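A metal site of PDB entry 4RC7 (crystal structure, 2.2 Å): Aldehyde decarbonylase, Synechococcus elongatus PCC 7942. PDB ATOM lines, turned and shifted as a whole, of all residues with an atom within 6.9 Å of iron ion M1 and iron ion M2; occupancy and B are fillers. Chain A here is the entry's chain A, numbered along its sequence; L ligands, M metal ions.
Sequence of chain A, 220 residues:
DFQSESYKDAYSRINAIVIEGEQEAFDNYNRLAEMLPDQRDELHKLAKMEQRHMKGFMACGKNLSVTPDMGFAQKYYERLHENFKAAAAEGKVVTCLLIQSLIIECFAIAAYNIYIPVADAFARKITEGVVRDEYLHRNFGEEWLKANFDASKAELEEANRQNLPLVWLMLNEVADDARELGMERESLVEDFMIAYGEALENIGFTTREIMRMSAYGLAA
Residues that only touch iron ion M1: Glu 134 (2.9 Å).
Within 4 Å of iron ion M1: Glu 22, Glu 50, His 53 and Glu 134.
The nearest printed residue that does not touch iron ion M1 is His 137 (4.5 Å).
OE1 of Glu 22 is bound to iron ion M1 (2.1 Å).
Iron ion M1 is bound by OE1 of Glu 50, 2.1 Å away.
ND1 of His 53 binds iron ion M1, 2.4 Å away.
Iron ion M2 is bound by the side-chain carboxylate (OE2) of Glu 50, the side-chain carboxylate (OE2) of Glu 105, a ring nitrogen (ND1) of His 137, an oxygen (O1) of the ligand and the side-chain carboxylate (OE1) of Glu 105.
Iron ion M2 has five donor atoms within binding distance.
Residues that only touch iron ion M2: Glu 134 (3.8 Å).
Four residues have an atom within 4 Å of iron ion M2: Glu 50, Glu 105, Glu 134 and His 137.
The nearest printed residue that does not touch iron ion M2 is Tyr 29 (4.2 Å).
An oxygen (O1) of the ligand lies close to the side-chain amide nitrogen of Gln 100, 3.5 Å away.
OH of Tyr 29 sits close to OE2 of Glu 105 (2.8 Å).
SD of Met 49 lies within hydrogen-bond range of NE2 of His 137, 3.5 Å away.
The backbone NH (N) of Glu 105 sits close to the backbone carbonyl oxygen (O) of Gln 100 (3.3 Å).
The side-chain hydroxyl (OH) of Tyr 112 is in hydrogen-bond range of the side-chain carboxylate (OE2) of Glu 22 (2.7 Å).
OE1 of Glu 105 lies close to OE1 of Glu 134, 2.7 Å away.
NE2 of His 53 sits at hydrogen-bond distance from OD2 of Asp 133.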
ATOM      1  N   GLY A  21     -22.078   6.189 -13.381  1.00  0.00           N
ATOM      2  CA  GLY A  21     -23.274   6.560 -12.617  1.00  0.00           C
ATOM      3  C   GLY A  21     -22.961   7.405 -11.402  1.00  0.00           C
ATOM      4  O   GLY A  21     -23.639   8.401 -11.140  1.00  0.00           O
ATOM      5  N   GLU A  22     -21.929   7.015 -10.652  1.00  0.00           N
ATOM      6  CA  GLU A  22     -21.536   7.756  -9.453  1.00  0.00           C
ATOM      7  C   GLU A  22     -21.024   9.147  -9.825  1.00  0.00           C
ATOM      8  O   GLU A  22     -21.309  10.132  -9.146  1.00  0.00           O
ATOM      9  CB  GLU A  22     -20.470   6.989  -8.665  1.00  0.00           C
ATOM     10  CG  GLU A  22     -20.891   5.599  -8.234  1.00  0.00           C
ATOM     11  CD  GLU A  22     -22.020   5.590  -7.198  1.00  0.00           C
ATOM     12  OE1 GLU A  22     -22.359   6.647  -6.625  1.00  0.00           O
ATOM     13  OE2 GLU A  22     -22.565   4.491  -6.937  1.00  0.00           O
ATOM     14  N   ALA A  25     -23.929  11.222 -10.707  1.00  0.00           N
ATOM     15  CA  ALA A  25     -24.612  11.546  -9.443  1.00  0.00           C
ATOM     16  C   ALA A  25     -23.896  12.708  -8.744  1.00  0.00           C
ATOM     17  O   ALA A  25     -24.527  13.651  -8.256  1.00  0.00           O
ATOM     18  CB  ALA A  25     -24.700  10.322  -8.539  1.00  0.00           C
ATOM     19  N   TYR A  29     -25.948  16.273  -8.102  1.00  0.00           N
ATOM     20  CA  TYR A  29     -26.233  16.843  -6.777  1.00  0.00           C
ATOM     21  C   TYR A  29     -25.589  18.221  -6.610  1.00  0.00           C
ATOM     22  O   TYR A  29     -26.175  19.087  -5.941  1.00  0.00           O
ATOM     23  CB  TYR A  29     -25.828  15.893  -5.637  1.00  0.00           C
ATOM     24  CG  TYR A  29     -26.819  14.774  -5.401  1.00  0.00           C
ATOM     25  CD1 TYR A  29     -28.141  15.042  -5.105  1.00  0.00           C
ATOM     26  CD2 TYR A  29     -26.420  13.436  -5.454  1.00  0.00           C
ATOM     27  CE1 TYR A  29     -29.051  14.027  -4.889  1.00  0.00           C
ATOM     28  CE2 TYR A  29     -27.314  12.404  -5.231  1.00  0.00           C
ATOM     29  CZ  TYR A  29     -28.626  12.697  -4.954  1.00  0.00           C
ATOM     30  OH  TYR A  29     -29.529  11.682  -4.726  1.00  0.00           O
ATOM     31  N   LEU A  46     -24.166  15.234  -0.112  1.00  0.00           N
ATOM     32  CA  LEU A  46     -24.580  14.101  -0.944  1.00  0.00           C
ATOM     33  C   LEU A  46     -23.616  13.933  -2.117  1.00  0.00           C
ATOM     34  O   LEU A  46     -23.124  12.832  -2.364  1.00  0.00           O
ATOM     35  CB  LEU A  46     -26.028  14.247  -1.442  1.00  0.00           C
ATOM     36  CG  LEU A  46     -27.108  14.399  -0.363  1.00  0.00           C
ATOM     37  CD1 LEU A  46     -28.527  14.341  -0.927  1.00  0.00           C
ATOM     38  CD2 LEU A  46     -26.946  13.391   0.764  1.00  0.00           C
ATOM     39  N   MET A  49     -20.377  12.316  -0.967  1.00  0.00           N
ATOM     40  CA  MET A  49     -20.609  10.871  -0.852  1.00  0.00           C
ATOM     41  C   MET A  49     -20.483  10.187  -2.238  1.00  0.00           C
ATOM     42  O   MET A  49     -19.828   9.163  -2.373  1.00  0.00           O
ATOM     43  CB  MET A  49     -21.953  10.536  -0.207  1.00  0.00           C
ATOM     44  CG  MET A  49     -22.067  10.925   1.260  1.00  0.00           C
ATOM     45  SD  MET A  49     -23.692  10.564   1.989  1.00  0.00           S
ATOM     46  CE  MET A  49     -24.007  12.058   2.920  1.00  0.00           C
ATOM     47  N   GLU A  50     -21.087  10.777  -3.270  1.00  0.00           N
ATOM     48  CA  GLU A  50     -20.999  10.176  -4.605  1.00  0.00           C
ATOM     49  C   GLU A  50     -19.533  10.028  -5.091  1.00  0.00           C
ATOM     50  O   GLU A  50     -19.152   8.990  -5.645  1.00  0.00           O
ATOM     51  CB  GLU A  50     -21.834  10.952  -5.634  1.00  0.00           C
ATOM     52  CG  GLU A  50     -23.300  11.154  -5.248  1.00  0.00           C
ATOM     53  CD  GLU A  50     -24.109   9.868  -5.132  1.00  0.00           C
ATOM     54  OE1 GLU A  50     -23.524   8.762  -5.220  1.00  0.00           O
ATOM     55  OE2 GLU A  50     -25.336   9.959  -4.939  1.00  0.00           O
ATOM     56  N   GLN A  51     -18.721  11.037  -4.847  1.00  0.00           N
ATOM     57  CA  GLN A  51     -17.303  10.991  -5.207  1.00  0.00           C
ATOM     58  C   GLN A  51     -16.606   9.818  -4.537  1.00  0.00           C
ATOM     59  O   GLN A  51     -15.796   9.145  -5.158  1.00  0.00           O
ATOM     60  CB  GLN A  51     -16.609  12.325  -4.877  1.00  0.00           C
ATOM     61  CG  GLN A  51     -15.099  12.331  -5.029  1.00  0.00           C
ATOM     62  CD  GLN A  51     -14.651  12.485  -6.462  1.00  0.00           C
ATOM     63  OE1 GLN A  51     -14.311  11.490  -7.119  1.00  0.00           O
ATOM     64  NE2 GLN A  51     -14.654  13.724  -6.963  1.00  0.00           N
ATOM     65  N   HIS A  53     -18.094   6.968  -3.538  1.00  0.00           N
ATOM     66  CA  HIS A  53     -18.586   5.767  -4.217  1.00  0.00           C
ATOM     67  C   HIS A  53     -17.832   5.515  -5.497  1.00  0.00           C
ATOM     68  O   HIS A  53     -17.434   4.392  -5.779  1.00  0.00           O
ATOM     69  CB  HIS A  53     -20.080   5.907  -4.515  1.00  0.00           C
ATOM     70  CG  HIS A  53     -20.926   6.150  -3.309  1.00  0.00           C
ATOM     71  ND1 HIS A  53     -22.214   6.483  -3.394  1.00  0.00           N
ATOM     72  CD2 HIS A  53     -20.620   6.100  -1.946  1.00  0.00           C
ATOM     73  CE1 HIS A  53     -22.734   6.636  -2.155  1.00  0.00           C
ATOM     74  NE2 HIS A  53     -21.745   6.409  -1.272  1.00  0.00           N
ATOM     75  N   MET A  54     -17.627   6.567  -6.280  1.00  0.00           N
ATOM     76  CA  MET A  54     -16.959   6.419  -7.556  1.00  0.00           C
ATOM     77  C   MET A  54     -15.567   5.833  -7.346  1.00  0.00           C
ATOM     78  O   MET A  54     -15.207   4.841  -7.974  1.00  0.00           O
ATOM     79  CB  MET A  54     -16.877   7.748  -8.299  1.00  0.00           C
ATOM     80  CG  MET A  54     -16.140   7.672  -9.637  1.00  0.00           C
ATOM     81  SD  MET A  54     -15.872   9.329 -10.256  1.00  0.00           S
ATOM     82  CE  MET A  54     -15.016   9.004 -11.804  1.00  0.00           C
ATOM     83  N   PHE A  57     -15.668   2.101  -6.368  1.00  0.00           N
ATOM     84  CA  PHE A  57     -15.916   1.175  -7.467  1.00  0.00           C
ATOM     85  C   PHE A  57     -14.786   1.106  -8.482  1.00  0.00           C
ATOM     86  O   PHE A  57     -14.593   0.079  -9.126  1.00  0.00           O
ATOM     87  CB  PHE A  57     -17.243   1.470  -8.136  1.00  0.00           C
ATOM     88  CG  PHE A  57     -18.418   1.133  -7.266  1.00  0.00           C
ATOM     89  CD1 PHE A  57     -18.612  -0.181  -6.830  1.00  0.00           C
ATOM     90  CD2 PHE A  57     -19.331   2.117  -6.879  1.00  0.00           C
ATOM     91  CE1 PHE A  57     -19.708  -0.507  -6.036  1.00  0.00           C
ATOM     92  CE2 PHE A  57     -20.405   1.790  -6.079  1.00  0.00           C
ATOM     93  CZ  PHE A  57     -20.592   0.472  -5.655  1.00  0.00           C
ATOM     94  N   GLN A 100     -32.621  12.033 -10.377  1.00  0.00           N
ATOM     95  CA  GLN A 100     -31.476  11.598  -9.572  1.00  0.00           C
ATOM     96  C   GLN A 100     -31.854  10.978  -8.214  1.00  0.00           C
ATOM     97  O   GLN A 100     -31.412   9.885  -7.915  1.00  0.00           O
ATOM     98  CB  GLN A 100     -30.442  12.713  -9.391  1.00  0.00           C
ATOM     99  CG  GLN A 100     -29.271  12.321  -8.479  1.00  0.00           C
ATOM    100  CD  GLN A 100     -28.459  11.158  -9.034  1.00  0.00           C
ATOM    101  OE1 GLN A 100     -28.060  11.163 -10.196  1.00  0.00           O
ATOM    102  NE2 GLN A 100     -28.210  10.158  -8.197  1.00  0.00           N
ATOM    103  N   ILE A 104     -33.058   7.174 -10.173  1.00  0.00           N
ATOM    104  CA  ILE A 104     -31.708   6.616 -10.177  1.00  0.00           C
ATOM    105  C   ILE A 104     -31.329   5.943  -8.847  1.00  0.00           C
ATOM    106  O   ILE A 104     -30.783   4.838  -8.854  1.00  0.00           O
ATOM    107  CB  ILE A 104     -30.647   7.662 -10.588  1.00  0.00           C
ATOM    108  CG1 ILE A 104     -30.752   7.974 -12.093  1.00  0.00           C
ATOM    109  CG2 ILE A 104     -29.236   7.128 -10.315  1.00  0.00           C
ATOM    110  CD1 ILE A 104     -29.839   9.119 -12.565  1.00  0.00           C
ATOM    111  N   GLU A 105     -31.603   6.592  -7.720  1.00  0.00           N
ATOM    112  CA  GLU A 105     -31.270   5.974  -6.422  1.00  0.00           C
ATOM    113  C   GLU A 105     -32.016   4.660  -6.212  1.00  0.00           C
ATOM    114  O   GLU A 105     -31.438   3.725  -5.723  1.00  0.00           O
ATOM    115  CB  GLU A 105     -31.537   6.912  -5.238  1.00  0.00           C
ATOM    116  CG  GLU A 105     -30.761   8.227  -5.235  1.00  0.00           C
ATOM    117  CD  GLU A 105     -29.260   8.067  -5.059  1.00  0.00           C
ATOM    118  OE1 GLU A 105     -28.772   6.973  -4.702  1.00  0.00           O
ATOM    119  OE2 GLU A 105     -28.569   9.080  -5.265  1.00  0.00           O
ATOM    120  N   ALA A 108     -30.290   2.017  -8.258  1.00  0.00           N
ATOM    121  CA  ALA A 108     -29.030   1.651  -7.606  1.00  0.00           C
ATOM    122  C   ALA A 108     -29.258   0.794  -6.364  1.00  0.00           C
ATOM    123  O   ALA A 108     -28.594  -0.205  -6.166  1.00  0.00           O
ATOM    124  CB  ALA A 108     -28.233   2.896  -7.256  1.00  0.00           C
ATOM    125  N   TYR A 112     -27.682  -2.846  -6.316  1.00  0.00           N
ATOM    126  CA  TYR A 112     -26.570  -3.032  -5.404  1.00  0.00           C
ATOM    127  C   TYR A 112     -26.910  -4.111  -4.363  1.00  0.00           C
ATOM    128  O   TYR A 112     -26.073  -4.958  -4.048  1.00  0.00           O
ATOM    129  CB  TYR A 112     -26.209  -1.721  -4.708  1.00  0.00           C
ATOM    130  CG  TYR A 112     -25.516  -0.689  -5.563  1.00  0.00           C
ATOM    131  CD1 TYR A 112     -25.044  -0.995  -6.829  1.00  0.00           C
ATOM    132  CD2 TYR A 112     -25.312   0.595  -5.091  1.00  0.00           C
ATOM    133  CE1 TYR A 112     -24.417  -0.048  -7.617  1.00  0.00           C
ATOM    134  CE2 TYR A 112     -24.673   1.558  -5.868  1.00  0.00           C
ATOM    135  CZ  TYR A 112     -24.226   1.224  -7.131  1.00  0.00           C
ATOM    136  OH  TYR A 112     -23.601   2.167  -7.910  1.00  0.00           O
ATOM    137  N   VAL A 130     -21.584   1.602   0.262  1.00  0.00           N
ATOM    138  CA  VAL A 130     -22.244   2.422  -0.723  1.00  0.00           C
ATOM    139  C   VAL A 130     -23.758   2.415  -0.538  1.00  0.00           C
ATOM    140  O   VAL A 130     -24.382   3.472  -0.448  1.00  0.00           O
ATOM    141  CB  VAL A 130     -21.857   1.985  -2.163  1.00  0.00           C
ATOM    142  CG1 VAL A 130     -22.791   2.572  -3.204  1.00  0.00           C
ATOM    143  CG2 VAL A 130     -20.433   2.428  -2.452  1.00  0.00           C
ATOM    144  N   ASP A 133     -25.379   4.764   2.046  1.00  0.00           N
ATOM    145  CA  ASP A 133     -25.568   6.162   1.604  1.00  0.00           C
ATOM    146  C   ASP A 133     -26.731   6.334   0.637  1.00  0.00           C
ATOM    147  O   ASP A 133     -27.402   7.343   0.670  1.00  0.00           O
ATOM    148  CB  ASP A 133     -24.326   6.745   0.935  1.00  0.00           C
ATOM    149  CG  ASP A 133     -23.088   6.650   1.798  1.00  0.00           C
ATOM    150  OD1 ASP A 133     -23.232   6.560   3.034  1.00  0.00           O
ATOM    151  OD2 ASP A 133     -21.974   6.655   1.222  1.00  0.00           O
ATOM    152  N   GLU A 134     -26.956   5.368  -0.247  1.00  0.00           N
ATOM    153  CA  GLU A 134     -28.044   5.476  -1.212  1.00  0.00           C
ATOM    154  C   GLU A 134     -29.410   5.649  -0.530  1.00  0.00           C
ATOM    155  O   GLU A 134     -30.245   6.431  -0.988  1.00  0.00           O
ATOM    156  CB  GLU A 134     -28.047   4.306  -2.213  1.00  0.00           C
ATOM    157  CG  GLU A 134     -26.656   3.944  -2.739  1.00  0.00           C
ATOM    158  CD  GLU A 134     -26.424   4.292  -4.206  1.00  0.00           C
ATOM    159  OE1 GLU A 134     -27.402   4.659  -4.896  1.00  0.00           O
ATOM    160  OE2 GLU A 134     -25.262   4.200  -4.689  1.00  0.00           O
ATOM    161  N   HIS A 137     -29.792   9.298   0.255  1.00  0.00           N
ATOM    162  CA  HIS A 137     -30.006  10.104  -0.947  1.00  0.00           C
ATOM    163  C   HIS A 137     -31.444  10.024  -1.400  1.00  0.00           C
ATOM    164  O   HIS A 137     -32.065  11.032  -1.696  1.00  0.00           O
ATOM    165  CB  HIS A 137     -29.090   9.625  -2.073  1.00  0.00           C
ATOM    166  CG  HIS A 137     -27.614   9.743  -1.785  1.00  0.00           C
ATOM    167  ND1 HIS A 137     -26.675   9.388  -2.678  1.00  0.00           N
ATOM    168  CD2 HIS A 137     -26.934  10.179  -0.641  1.00  0.00           C
ATOM    169  CE1 HIS A 137     -25.453   9.570  -2.121  1.00  0.00           C
ATOM    170  NE2 HIS A 137     -25.620  10.061  -0.892  1.00  0.00           N
ATOM    171  N   ARG A 138     -31.993   8.806  -1.467  1.00  0.00           N
ATOM    172  CA  ARG A 138     -33.406   8.626  -1.779  1.00  0.00           C
ATOM    173  C   ARG A 138     -34.301   9.321  -0.727  1.00  0.00           C
ATOM    174  O   ARG A 138     -35.290   9.968  -1.086  1.00  0.00           O
ATOM    175  CB  ARG A 138     -33.741   7.137  -1.882  1.00  0.00           C
ATOM    176  CG  ARG A 138     -35.193   6.820  -2.256  1.00  0.00           C
ATOM    177  CD  ARG A 138     -35.621   5.466  -1.719  1.00  0.00           C
ATOM    178  NE  ARG A 138     -35.413   5.401  -0.264  1.00  0.00           N
ATOM    179  CZ  ARG A 138     -35.272   4.287   0.457  1.00  0.00           C
ATOM    180  NH1 ARG A 138     -35.320   3.101  -0.110  1.00  0.00           N
ATOM    181  NH2 ARG A 138     -35.074   4.391   1.772  1.00  0.00           N
HETATM  182  C1  LIG L   1     -25.677   6.650  -7.595  1.00  0.00           C
HETATM  183  O1  LIG L   1     -26.340   7.478  -6.953  1.00  0.00           O
HETATM  184  C2  LIG L   1     -26.147   6.309  -8.991  1.00  0.00           C
HETATM  185  C3  LIG L   1     -25.526   5.016  -9.498  1.00  0.00           C
HETATM  186  C4  LIG L   1     -26.507   4.267 -10.415  1.00  0.00           C
HETATM  187  C5  LIG L   1     -25.833   2.984 -10.970  1.00  0.00           C
HETATM  188  C6  LIG L   1     -26.890   1.938 -11.342  1.00  0.00           C
HETATM  189  C7  LIG L   1     -26.275   0.840 -12.224  1.00  0.00           C
HETATM  190  C8  LIG L   1     -27.155  -0.406 -12.302  1.00  0.00           C
HETATM  191  C9  LIG L   1     -26.592  -1.411 -13.314  1.00  0.00           C
HETATM  192  C10 LIG L   1     -26.104  -2.737 -12.713  1.00  0.00           C
HETATM  193  C11 LIG L   1     -25.741  -2.668 -11.234  1.00  0.00           C
HETATM  194  C12 LIG L   1     -24.355  -3.230 -10.958  1.00  0.00           C
HETATM  195  C13 LIG L   1     -24.112  -3.545  -9.486  1.00  0.00           C
HETATM  196  C14 LIG L   1     -22.691  -4.063  -9.327  1.00  0.00           C
HETATM  197  C15 LIG L   1     -21.745  -2.991  -8.746  1.00  0.00           C
HETATM  198  C16 LIG L   1     -20.292  -3.316  -9.113  1.00  0.00           C
HETATM  199 FE    FE M   1     -23.805   6.662  -5.152  1.00  0.00          FE
HETATM  200 FE    FE M   2     -26.596   8.328  -4.706  1.00  0.00          FE
